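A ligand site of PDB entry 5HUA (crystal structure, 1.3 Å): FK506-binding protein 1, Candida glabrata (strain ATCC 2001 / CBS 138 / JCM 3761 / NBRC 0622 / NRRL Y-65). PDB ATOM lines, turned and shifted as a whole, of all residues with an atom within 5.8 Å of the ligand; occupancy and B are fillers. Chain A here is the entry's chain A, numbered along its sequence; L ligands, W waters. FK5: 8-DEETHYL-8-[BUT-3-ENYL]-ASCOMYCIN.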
ATOM      1  N   TYR A  34      11.514  13.037  -9.000  1.00  0.00           N
ATOM      2  CA  TYR A  34      12.851  13.537  -9.224  1.00  0.00           C
ATOM      3  C   TYR A  34      13.144  14.833  -8.505  1.00  0.00           C
ATOM      4  O   TYR A  34      12.192  15.610  -8.221  1.00  0.00           O
ATOM      5  CB  TYR A  34      13.139  13.781 -10.728  1.00  0.00           C
ATOM      6  CG  TYR A  34      12.392  14.902 -11.347  1.00  0.00           C
ATOM      7  CD1 TYR A  34      12.905  16.194 -11.359  1.00  0.00           C
ATOM      8  CD2 TYR A  34      11.112  14.739 -11.886  1.00  0.00           C
ATOM      9  CE1 TYR A  34      12.210  17.220 -11.903  1.00  0.00           C
ATOM     10  CE2 TYR A  34      10.434  15.780 -12.447  1.00  0.00           C
ATOM     11  CZ  TYR A  34      10.970  17.031 -12.459  1.00  0.00           C
ATOM     12  OH  TYR A  34      10.272  18.069 -13.031  1.00  0.00           O
ATOM     13  N   GLY A  36      16.053  17.884  -9.455  1.00  0.00           N
ATOM     14  CA  GLY A  36      17.111  18.306 -10.365  1.00  0.00           C
ATOM     15  C   GLY A  36      17.940  19.415  -9.762  1.00  0.00           C
ATOM     16  O   GLY A  36      17.370  20.410  -9.226  1.00  0.00           O
ATOM     17  N   PHE A  44      16.987  23.239  -9.073  1.00  0.00           N
ATOM     18  CA  PHE A  44      16.165  23.980 -10.026  1.00  0.00           C
ATOM     19  C   PHE A  44      14.726  23.485 -10.061  1.00  0.00           C
ATOM     20  O   PHE A  44      13.847  24.240 -10.485  1.00  0.00           O
ATOM     21  CB  PHE A  44      16.802  24.100 -11.404  1.00  0.00           C
ATOM     22  CG  PHE A  44      17.046  22.780 -12.091  1.00  0.00           C
ATOM     23  CD1 PHE A  44      16.018  22.143 -12.787  1.00  0.00           C
ATOM     24  CD2 PHE A  44      18.268  22.168 -12.044  1.00  0.00           C
ATOM     25  CE1 PHE A  44      16.246  20.925 -13.411  1.00  0.00           C
ATOM     26  CE2 PHE A  44      18.482  20.967 -12.692  1.00  0.00           C
ATOM     27  CZ  PHE A  44      17.456  20.372 -13.349  1.00  0.00           C
ATOM     28  N   ASP A  45      14.464  22.216  -9.733  1.00  0.00           N
ATOM     29  CA  ASP A  45      13.110  21.699  -9.797  1.00  0.00           C
ATOM     30  C   ASP A  45      12.994  20.441  -9.056  1.00  0.00           C
ATOM     31  O   ASP A  45      14.001  19.732  -8.817  1.00  0.00           O
ATOM     32  CB  ASP A  45      12.684  21.500 -11.258  1.00  0.00           C
ATOM     33  CG  ASP A  45      11.243  21.188 -11.431  1.00  0.00           C
ATOM     34  OD1 ASP A  45      10.419  21.598 -10.565  1.00  0.00           O
ATOM     35  OD2 ASP A  45      10.867  20.566 -12.472  1.00  0.00           O
ATOM     36  N   ARG A  50       6.057  19.454  -5.764  1.00  0.00           N
ATOM     37  CA  ARG A  50       4.700  19.567  -6.293  1.00  0.00           C
ATOM     38  C   ARG A  50       3.702  18.552  -5.718  1.00  0.00           C
ATOM     39  O   ARG A  50       2.521  18.588  -6.045  1.00  0.00           O
ATOM     40  CB  ARG A  50       4.643  19.461  -7.857  1.00  0.00           C
ATOM     41  CG  ARG A  50       5.285  20.613  -8.575  1.00  0.00           C
ATOM     42  CD  ARG A  50       5.089  20.465 -10.068  1.00  0.00           C
ATOM     43  NE  ARG A  50       5.871  19.387 -10.687  1.00  0.00           N
ATOM     44  CZ  ARG A  50       7.134  19.541 -10.980  1.00  0.00           C
ATOM     45  NH1 ARG A  50       7.694  20.699 -10.664  1.00  0.00           N
ATOM     46  NH2 ARG A  50       7.765  18.585 -11.585  1.00  0.00           N
ATOM     47  N   PHE A  54       6.082  12.610 -11.692  1.00  0.00           N
ATOM     48  CA  PHE A  54       6.194  12.868 -13.148  1.00  0.00           C
ATOM     49  C   PHE A  54       5.940  11.600 -13.910  1.00  0.00           C
ATOM     50  O   PHE A  54       6.398  10.546 -13.556  1.00  0.00           O
ATOM     51  CB  PHE A  54       7.550  13.436 -13.400  1.00  0.00           C
ATOM     52  CG  PHE A  54       7.837  13.659 -14.876  1.00  0.00           C
ATOM     53  CD1 PHE A  54       7.189  14.645 -15.572  1.00  0.00           C
ATOM     54  CD2 PHE A  54       8.705  12.848 -15.565  1.00  0.00           C
ATOM     55  CE1 PHE A  54       7.434  14.820 -16.955  1.00  0.00           C
ATOM     56  CE2 PHE A  54       8.919  13.057 -16.939  1.00  0.00           C
ATOM     57  CZ  PHE A  54       8.293  14.034 -17.596  1.00  0.00           C
ATOM     58  N   GLN A  62      10.279  12.284 -25.551  1.00  0.00           N
ATOM     59  CA  GLN A  62       9.477  13.210 -24.744  1.00  0.00           C
ATOM     60  C   GLN A  62      10.325  14.014 -23.814  1.00  0.00           C
ATOM     61  O   GLN A  62       9.907  15.111 -23.354  1.00  0.00           O
ATOM     62  CB  GLN A  62       8.423  12.475 -23.925  1.00  0.00           C
ATOM     63  CG  GLN A  62       7.233  11.975 -24.734  1.00  0.00           C
ATOM     64  CD  GLN A  62       6.275  11.182 -23.940  1.00  0.00           C
ATOM     65  OE1 GLN A  62       6.341  11.111 -22.661  1.00  0.00           O
ATOM     66  NE2 GLN A  62       5.308  10.587 -24.552  1.00  0.00           N
ATOM     67  N   VAL A  63      11.455  13.483 -23.392  1.00  0.00           N
ATOM     68  CA  VAL A  63      12.293  14.056 -22.354  1.00  0.00           C
ATOM     69  C   VAL A  63      13.686  14.179 -22.896  1.00  0.00           C
ATOM     70  O   VAL A  63      14.011  13.628 -23.983  1.00  0.00           O
ATOM     71  CB  VAL A  63      12.235  13.186 -21.081  1.00  0.00           C
ATOM     72  CG1 VAL A  63      10.855  13.305 -20.458  1.00  0.00           C
ATOM     73  CG2 VAL A  63      12.618  11.739 -21.351  1.00  0.00           C
ATOM     74  N   ILE A  64      14.554  14.856 -22.184  1.00  0.00           N
ATOM     75  CA  ILE A  64      15.933  15.028 -22.545  1.00  0.00           C
ATOM     76  C   ILE A  64      16.607  13.695 -22.732  1.00  0.00           C
ATOM     77  O   ILE A  64      16.281  12.656 -22.139  1.00  0.00           O
ATOM     78  CB  ILE A  64      16.697  15.929 -21.568  1.00  0.00           C
ATOM     79  CG1 ILE A  64      16.637  15.382 -20.145  1.00  0.00           C
ATOM     80  CG2 ILE A  64      16.208  17.382 -21.666  1.00  0.00           C
ATOM     81  CD1 ILE A  64      17.534  16.146 -19.142  1.00  0.00           C
ATOM     82  N   TRP A  67      17.653  11.357 -19.833  1.00  0.00           N
ATOM     83  CA  TRP A  67      16.586  10.562 -19.219  1.00  0.00           C
ATOM     84  C   TRP A  67      16.247   9.358 -20.081  1.00  0.00           C
ATOM     85  O   TRP A  67      16.080   8.236 -19.566  1.00  0.00           O
ATOM     86  CB  TRP A  67      15.334  11.401 -18.959  1.00  0.00           C
ATOM     87  CG  TRP A  67      15.329  12.162 -17.664  1.00  0.00           C
ATOM     88  CD1 TRP A  67      16.273  13.001 -17.181  1.00  0.00           C
ATOM     89  CD2 TRP A  67      14.308  12.091 -16.684  1.00  0.00           C
ATOM     90  NE1 TRP A  67      15.897  13.497 -15.935  1.00  0.00           N
ATOM     91  CE2 TRP A  67      14.672  12.943 -15.644  1.00  0.00           C
ATOM     92  CE3 TRP A  67      13.088  11.394 -16.617  1.00  0.00           C
ATOM     93  CZ2 TRP A  67      13.836  13.123 -14.496  1.00  0.00           C
ATOM     94  CZ3 TRP A  67      12.271  11.599 -15.500  1.00  0.00           C
ATOM     95  CH2 TRP A  67      12.665  12.461 -14.480  1.00  0.00           C
ATOM     96  N   ALA A  89      21.311  17.101 -22.312  1.00  0.00           N
ATOM     97  CA  ALA A  89      20.335  17.879 -21.536  1.00  0.00           C
ATOM     98  C   ALA A  89      19.909  19.036 -22.390  1.00  0.00           C
ATOM     99  O   ALA A  89      19.331  18.780 -23.467  1.00  0.00           O
ATOM    100  CB  ALA A  89      20.953  18.260 -20.182  1.00  0.00           C
ATOM    101  N   TYR A  90      20.184  20.293 -22.026  1.00  0.00           N
ATOM    102  CA  TYR A  90      19.657  21.446 -22.749  1.00  0.00           C
ATOM    103  C   TYR A  90      20.674  22.152 -23.606  1.00  0.00           C
ATOM    104  O   TYR A  90      20.365  23.190 -24.212  1.00  0.00           O
ATOM    105  CB  TYR A  90      18.949  22.412 -21.778  1.00  0.00           C
ATOM    106  CG  TYR A  90      17.719  21.808 -21.150  1.00  0.00           C
ATOM    107  CD1 TYR A  90      16.502  21.943 -21.744  1.00  0.00           C
ATOM    108  CD2 TYR A  90      17.804  21.065 -19.999  1.00  0.00           C
ATOM    109  CE1 TYR A  90      15.368  21.301 -21.204  1.00  0.00           C
ATOM    110  CE2 TYR A  90      16.694  20.447 -19.427  1.00  0.00           C
ATOM    111  CZ  TYR A  90      15.510  20.578 -20.072  1.00  0.00           C
ATOM    112  OH  TYR A  90      14.366  19.930 -19.560  1.00  0.00           O
ATOM    113  N   GLY A  91      21.899  21.625 -23.683  1.00  0.00           N
ATOM    114  CA  GLY A  91      22.848  22.098 -24.704  1.00  0.00           C
ATOM    115  C   GLY A  91      23.218  23.554 -24.518  1.00  0.00           C
ATOM    116  O   GLY A  91      23.157  24.132 -23.414  1.00  0.00           O
ATOM    117  N   ARG A  93      21.720  26.175 -25.422  1.00  0.00           N
ATOM    118  CA  ARG A  93      20.581  27.056 -25.177  1.00  0.00           C
ATOM    119  C   ARG A  93      20.161  27.120 -23.715  1.00  0.00           C
ATOM    120  O   ARG A  93      19.804  28.226 -23.245  1.00  0.00           O
ATOM    121  CB  ARG A  93      19.415  26.644 -26.028  1.00  0.00           C
ATOM    122  CG  ARG A  93      18.198  27.479 -25.899  1.00  0.00           C
ATOM    123  CD  ARG A  93      17.142  27.141 -26.892  1.00  0.00           C
ATOM    124  NE  ARG A  93      17.606  27.511 -28.228  1.00  0.00           N
ATOM    125  CZ  ARG A  93      17.059  27.061 -29.349  1.00  0.00           C
ATOM    126  NH1 ARG A  93      16.024  26.218 -29.283  1.00  0.00           N
ATOM    127  NH2 ARG A  93      17.542  27.435 -30.522  1.00  0.00           N
ATOM    128  N   PHE A  95      17.604  26.671 -20.497  1.00  0.00           N
ATOM    129  CA  PHE A  95      16.156  26.824 -20.298  1.00  0.00           C
ATOM    130  C   PHE A  95      15.963  28.073 -19.389  1.00  0.00           C
ATOM    131  O   PHE A  95      16.578  28.131 -18.328  1.00  0.00           O
ATOM    132  CB  PHE A  95      15.523  25.583 -19.625  1.00  0.00           C
ATOM    133  CG  PHE A  95      14.048  25.670 -19.615  1.00  0.00           C
ATOM    134  CD1 PHE A  95      13.371  26.399 -18.655  1.00  0.00           C
ATOM    135  CD2 PHE A  95      13.306  25.082 -20.617  1.00  0.00           C
ATOM    136  CE1 PHE A  95      11.969  26.554 -18.713  1.00  0.00           C
ATOM    137  CE2 PHE A  95      11.908  25.247 -20.639  1.00  0.00           C
ATOM    138  CZ  PHE A  95      11.309  25.967 -19.725  1.00  0.00           C
ATOM    139  N   LEU A  98      16.039  28.520 -15.254  1.00  0.00           N
ATOM    140  CA  LEU A  98      16.333  27.242 -14.613  1.00  0.00           C
ATOM    141  C   LEU A  98      17.677  26.677 -14.966  1.00  0.00           C
ATOM    142  O   LEU A  98      18.381  26.197 -14.083  1.00  0.00           O
ATOM    143  CB  LEU A  98      15.260  26.218 -14.952  1.00  0.00           C
ATOM    144  CG  LEU A  98      13.858  26.591 -14.470  1.00  0.00           C
ATOM    145  CD1 LEU A  98      12.852  25.593 -14.989  1.00  0.00           C
ATOM    146  CD2 LEU A  98      13.751  26.728 -12.926  1.00  0.00           C
ATOM    147  N   ILE A  99      18.028  26.673 -16.270  1.00  0.00           N
ATOM    148  CA  ILE A  99      19.187  25.869 -16.710  1.00  0.00           C
ATOM    149  C   ILE A  99      20.095  26.820 -17.546  1.00  0.00           C
ATOM    150  O   ILE A  99      19.686  27.293 -18.610  1.00  0.00           O
ATOM    151  CB  ILE A  99      18.777  24.692 -17.584  1.00  0.00           C
ATOM    152  CG1 ILE A  99      17.656  23.746 -17.049  1.00  0.00           C
ATOM    153  CG2 ILE A  99      19.999  23.917 -18.006  1.00  0.00           C
ATOM    154  CD1 ILE A  99      18.017  23.185 -15.851  1.00  0.00           C
ATOM    155  N   LEU A 105      23.607  18.475 -15.585  1.00  0.00           N
ATOM    156  CA  LEU A 105      22.494  18.418 -14.649  1.00  0.00           C
ATOM    157  C   LEU A 105      22.593  17.163 -13.832  1.00  0.00           C
ATOM    158  O   LEU A 105      22.989  16.096 -14.300  1.00  0.00           O
ATOM    159  CB  LEU A 105      21.155  18.395 -15.396  1.00  0.00           C
ATOM    160  CG  LEU A 105      20.938  19.566 -16.367  1.00  0.00           C
ATOM    161  CD1 LEU A 105      19.532  19.484 -16.915  1.00  0.00           C
ATOM    162  CD2 LEU A 105      21.178  20.860 -15.701  1.00  0.00           C
ATOM    163  N   PHE A 107      20.168  14.662 -11.610  1.00  0.00           N
ATOM    164  CA  PHE A 107      18.825  14.293 -11.207  1.00  0.00           C
ATOM    165  C   PHE A 107      18.877  13.132 -10.285  1.00  0.00           C
ATOM    166  O   PHE A 107      19.404  12.069 -10.607  1.00  0.00           O
ATOM    167  CB  PHE A 107      17.953  13.894 -12.397  1.00  0.00           C
ATOM    168  CG  PHE A 107      17.553  15.029 -13.266  1.00  0.00           C
ATOM    169  CD1 PHE A 107      16.334  15.683 -13.086  1.00  0.00           C
ATOM    170  CD2 PHE A 107      18.336  15.438 -14.357  1.00  0.00           C
ATOM    171  CE1 PHE A 107      15.936  16.690 -13.936  1.00  0.00           C
ATOM    172  CE2 PHE A 107      17.921  16.440 -15.204  1.00  0.00           C
ATOM    173  CZ  PHE A 107      16.734  17.060 -14.997  1.00  0.00           C
HETATM  174  C1  FK5 L   1      12.473  17.114 -19.337  1.00  0.00           C
HETATM  175  C2  FK5 L   1      13.261  16.914 -18.081  1.00  0.00           C
HETATM  176  C3  FK5 L   1      13.296  15.445 -17.652  1.00  0.00           C
HETATM  177  C4  FK5 L   1      11.943  14.985 -17.116  1.00  0.00           C
HETATM  178  C5  FK5 L   1      11.488  15.854 -15.954  1.00  0.00           C
HETATM  179  C6  FK5 L   1      11.431  17.321 -16.371  1.00  0.00           C
HETATM  180  C8  FK5 L   1      13.402  18.746 -16.524  1.00  0.00           C
HETATM  181  C9  FK5 L   1      13.008  19.569 -15.480  1.00  0.00           C
HETATM  182  C10 FK5 L   1      12.195  20.825 -15.698  1.00  0.00           C
HETATM  183  C11 FK5 L   1      12.559  21.599 -16.973  1.00  0.00           C
HETATM  184  C12 FK5 L   1      11.473  22.627 -17.308  1.00  0.00           C
HETATM  185  C13 FK5 L   1      10.085  21.995 -17.271  1.00  0.00           C
HETATM  186  C14 FK5 L   1       9.888  21.340 -15.914  1.00  0.00           C
HETATM  187  C15 FK5 L   1       8.545  20.638 -15.682  1.00  0.00           C
HETATM  188  C16 FK5 L   1       8.141  19.747 -16.854  1.00  0.00           C
HETATM  189  C17 FK5 L   1       6.921  18.859 -16.555  1.00  0.00           C
HETATM  190  C18 FK5 L   1       5.615  19.587 -16.866  1.00  0.00           C
HETATM  191  C19 FK5 L   1       5.329  19.559 -18.344  1.00  0.00           C
HETATM  192  C20 FK5 L   1       5.728  20.708 -19.155  1.00  0.00           C
HETATM  193  C21 FK5 L   1       5.571  20.738 -20.643  1.00  0.00           C
HETATM  194  C22 FK5 L   1       6.871  20.264 -21.218  1.00  0.00           C
HETATM  195  C23 FK5 L   1       7.051  18.809 -21.546  1.00  0.00           C
HETATM  196  C24 FK5 L   1       8.481  18.373 -21.784  1.00  0.00           C
HETATM  197  C25 FK5 L   1       9.275  18.214 -20.475  1.00  0.00           C
HETATM  198  C26 FK5 L   1      10.794  17.990 -20.687  1.00  0.00           C
HETATM  199  C27 FK5 L   1      11.371  19.113 -21.495  1.00  0.00           C
HETATM  200  C28 FK5 L   1      11.928  18.782 -22.805  1.00  0.00           C
HETATM  201  C29 FK5 L   1      12.490  19.824 -23.732  1.00  0.00           C
HETATM  202  C30 FK5 L   1      13.844  19.330 -24.248  1.00  0.00           C
HETATM  203  C31 FK5 L   1      14.416  20.292 -25.293  1.00  0.00           C
HETATM  204  C32 FK5 L   1      13.438  20.567 -26.429  1.00  0.00           C
HETATM  205  C33 FK5 L   1      12.088  21.038 -25.893  1.00  0.00           C
HETATM  206  C34 FK5 L   1      11.530  20.027 -24.900  1.00  0.00           C
HETATM  207  C35 FK5 L   1      13.927  22.282 -16.892  1.00  0.00           C
HETATM  208  C36 FK5 L   1       6.918  18.365 -15.112  1.00  0.00           C
HETATM  209  C37 FK5 L   1       4.619  18.382 -18.956  1.00  0.00           C
HETATM  210  C38 FK5 L   1       5.250  22.178 -21.018  1.00  0.00           C
HETATM  211  C39 FK5 L   1       5.314  22.380 -22.512  1.00  0.00           C
HETATM  212  C40 FK5 L   1       4.792  21.354 -23.415  1.00  0.00           C
HETATM  213  C41 FK5 L   1       8.706  17.078 -19.648  1.00  0.00           C
HETATM  214  C42 FK5 L   1      11.345  20.509 -20.959  1.00  0.00           C
HETATM  215  C43 FK5 L   1       8.912  23.275 -18.845  1.00  0.00           C
HETATM  216  C44 FK5 L   1       7.477  21.962 -14.060  1.00  0.00           C
HETATM  217  C45 FK5 L   1      16.730  20.086 -25.061  1.00  0.00           C
HETATM  218  N7  FK5 L   1      12.708  17.714 -16.983  1.00  0.00           N
HETATM  219  O1  FK5 L   1      11.479  17.884 -19.430  1.00  0.00           O
HETATM  220  O2  FK5 L   1      12.881  16.360 -20.400  1.00  0.00           O
HETATM  221  O3  FK5 L   1      14.617  19.066 -17.084  1.00  0.00           O
HETATM  222  O4  FK5 L   1      13.431  19.199 -14.208  1.00  0.00           O
HETATM  223  O5  FK5 L   1      10.881  20.346 -15.759  1.00  0.00           O
HETATM  224  O6  FK5 L   1      12.354  21.715 -14.574  1.00  0.00           O
HETATM  225  O7  FK5 L   1       9.106  22.983 -17.487  1.00  0.00           O
HETATM  226  O8  FK5 L   1       7.528  21.580 -15.415  1.00  0.00           O
HETATM  227  O9  FK5 L   1       7.917  21.156 -21.443  1.00  0.00           O
HETATM  228  O10 FK5 L   1       8.352  17.143 -22.448  1.00  0.00           O
HETATM  229  O11 FK5 L   1      15.611  19.752 -25.844  1.00  0.00           O
HETATM  230  O12 FK5 L   1      13.953  21.552 -27.300  1.00  0.00           O
HETATM  231  O   HOH W   1       5.922  23.500 -16.728  1.00  0.00           O
HETATM  232  O   HOH W   2       9.003  24.976 -15.566  1.00  0.00           O
HETATM  233  O   HOH W   3      12.246  21.822 -29.634  1.00  0.00           O
HETATM  234  O   HOH W   4      13.923  23.407 -24.092  1.00  0.00           O
HETATM  235  O   HOH W   5      16.658  20.951 -28.353  1.00  0.00           O
HETATM  236  O   HOH W   6      16.278  16.909 -26.241  1.00  0.00           O
HETATM  237  O   HOH W   7       8.295  21.948 -23.939  1.00  0.00           O
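Residues that only touch the ligand: Val 63, Tyr 34, Ala 89, Phe 44, Trp 67, Phe 107, Phe 54, Arg 50, Phe 95 and Leu 98.
Along chain A the residues within 4 Å of the ligand span positions 34 to 107.
The nearest printed residue that does not touch the ligand is Ile 99 (4.01 Å).
The side-chain hydroxyl (OH) of Tyr 34 is in hydrogen-bond range of the guanidinium group (NH2) of Arg 50 (2.9 Å).
The backbone NH (N) of Phe 44 is in hydrogen-bond range of the backbone carbonyl oxygen (O) of Gly 36 (2.9 Å).
The backbone carbonyl oxygen of Asp 45 lies within hydrogen-bond range of the backbone NH of Gly 36 (2.8 Å).
The guanidinium group (NH1) of Arg 50 is in salt-bridge range of the side-chain carboxylate (OD1) of Asp 45 (2.9 Å).
The side-chain hydroxyl (OH) of Tyr 34 is in hydrogen-bond range of the side-chain carboxylate (OD2) of Asp 45, 2.6 Å away.
N of Ile 64 lies within hydrogen-bond range of O2 of the ligand, at 2.9 Å.
The side-chain carboxylate of Asp 45 is in hydrogen-bond range of an oxygen (O6) of the ligand (2.8 Å).
O10 of the ligand sits at hydrogen-bond distance from O of Gln 62 (2.7 Å).
The side-chain hydroxyl (OH) of Tyr 90 sits at hydrogen-bond distance from an oxygen (O3) of the ligand (2.6 Å).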
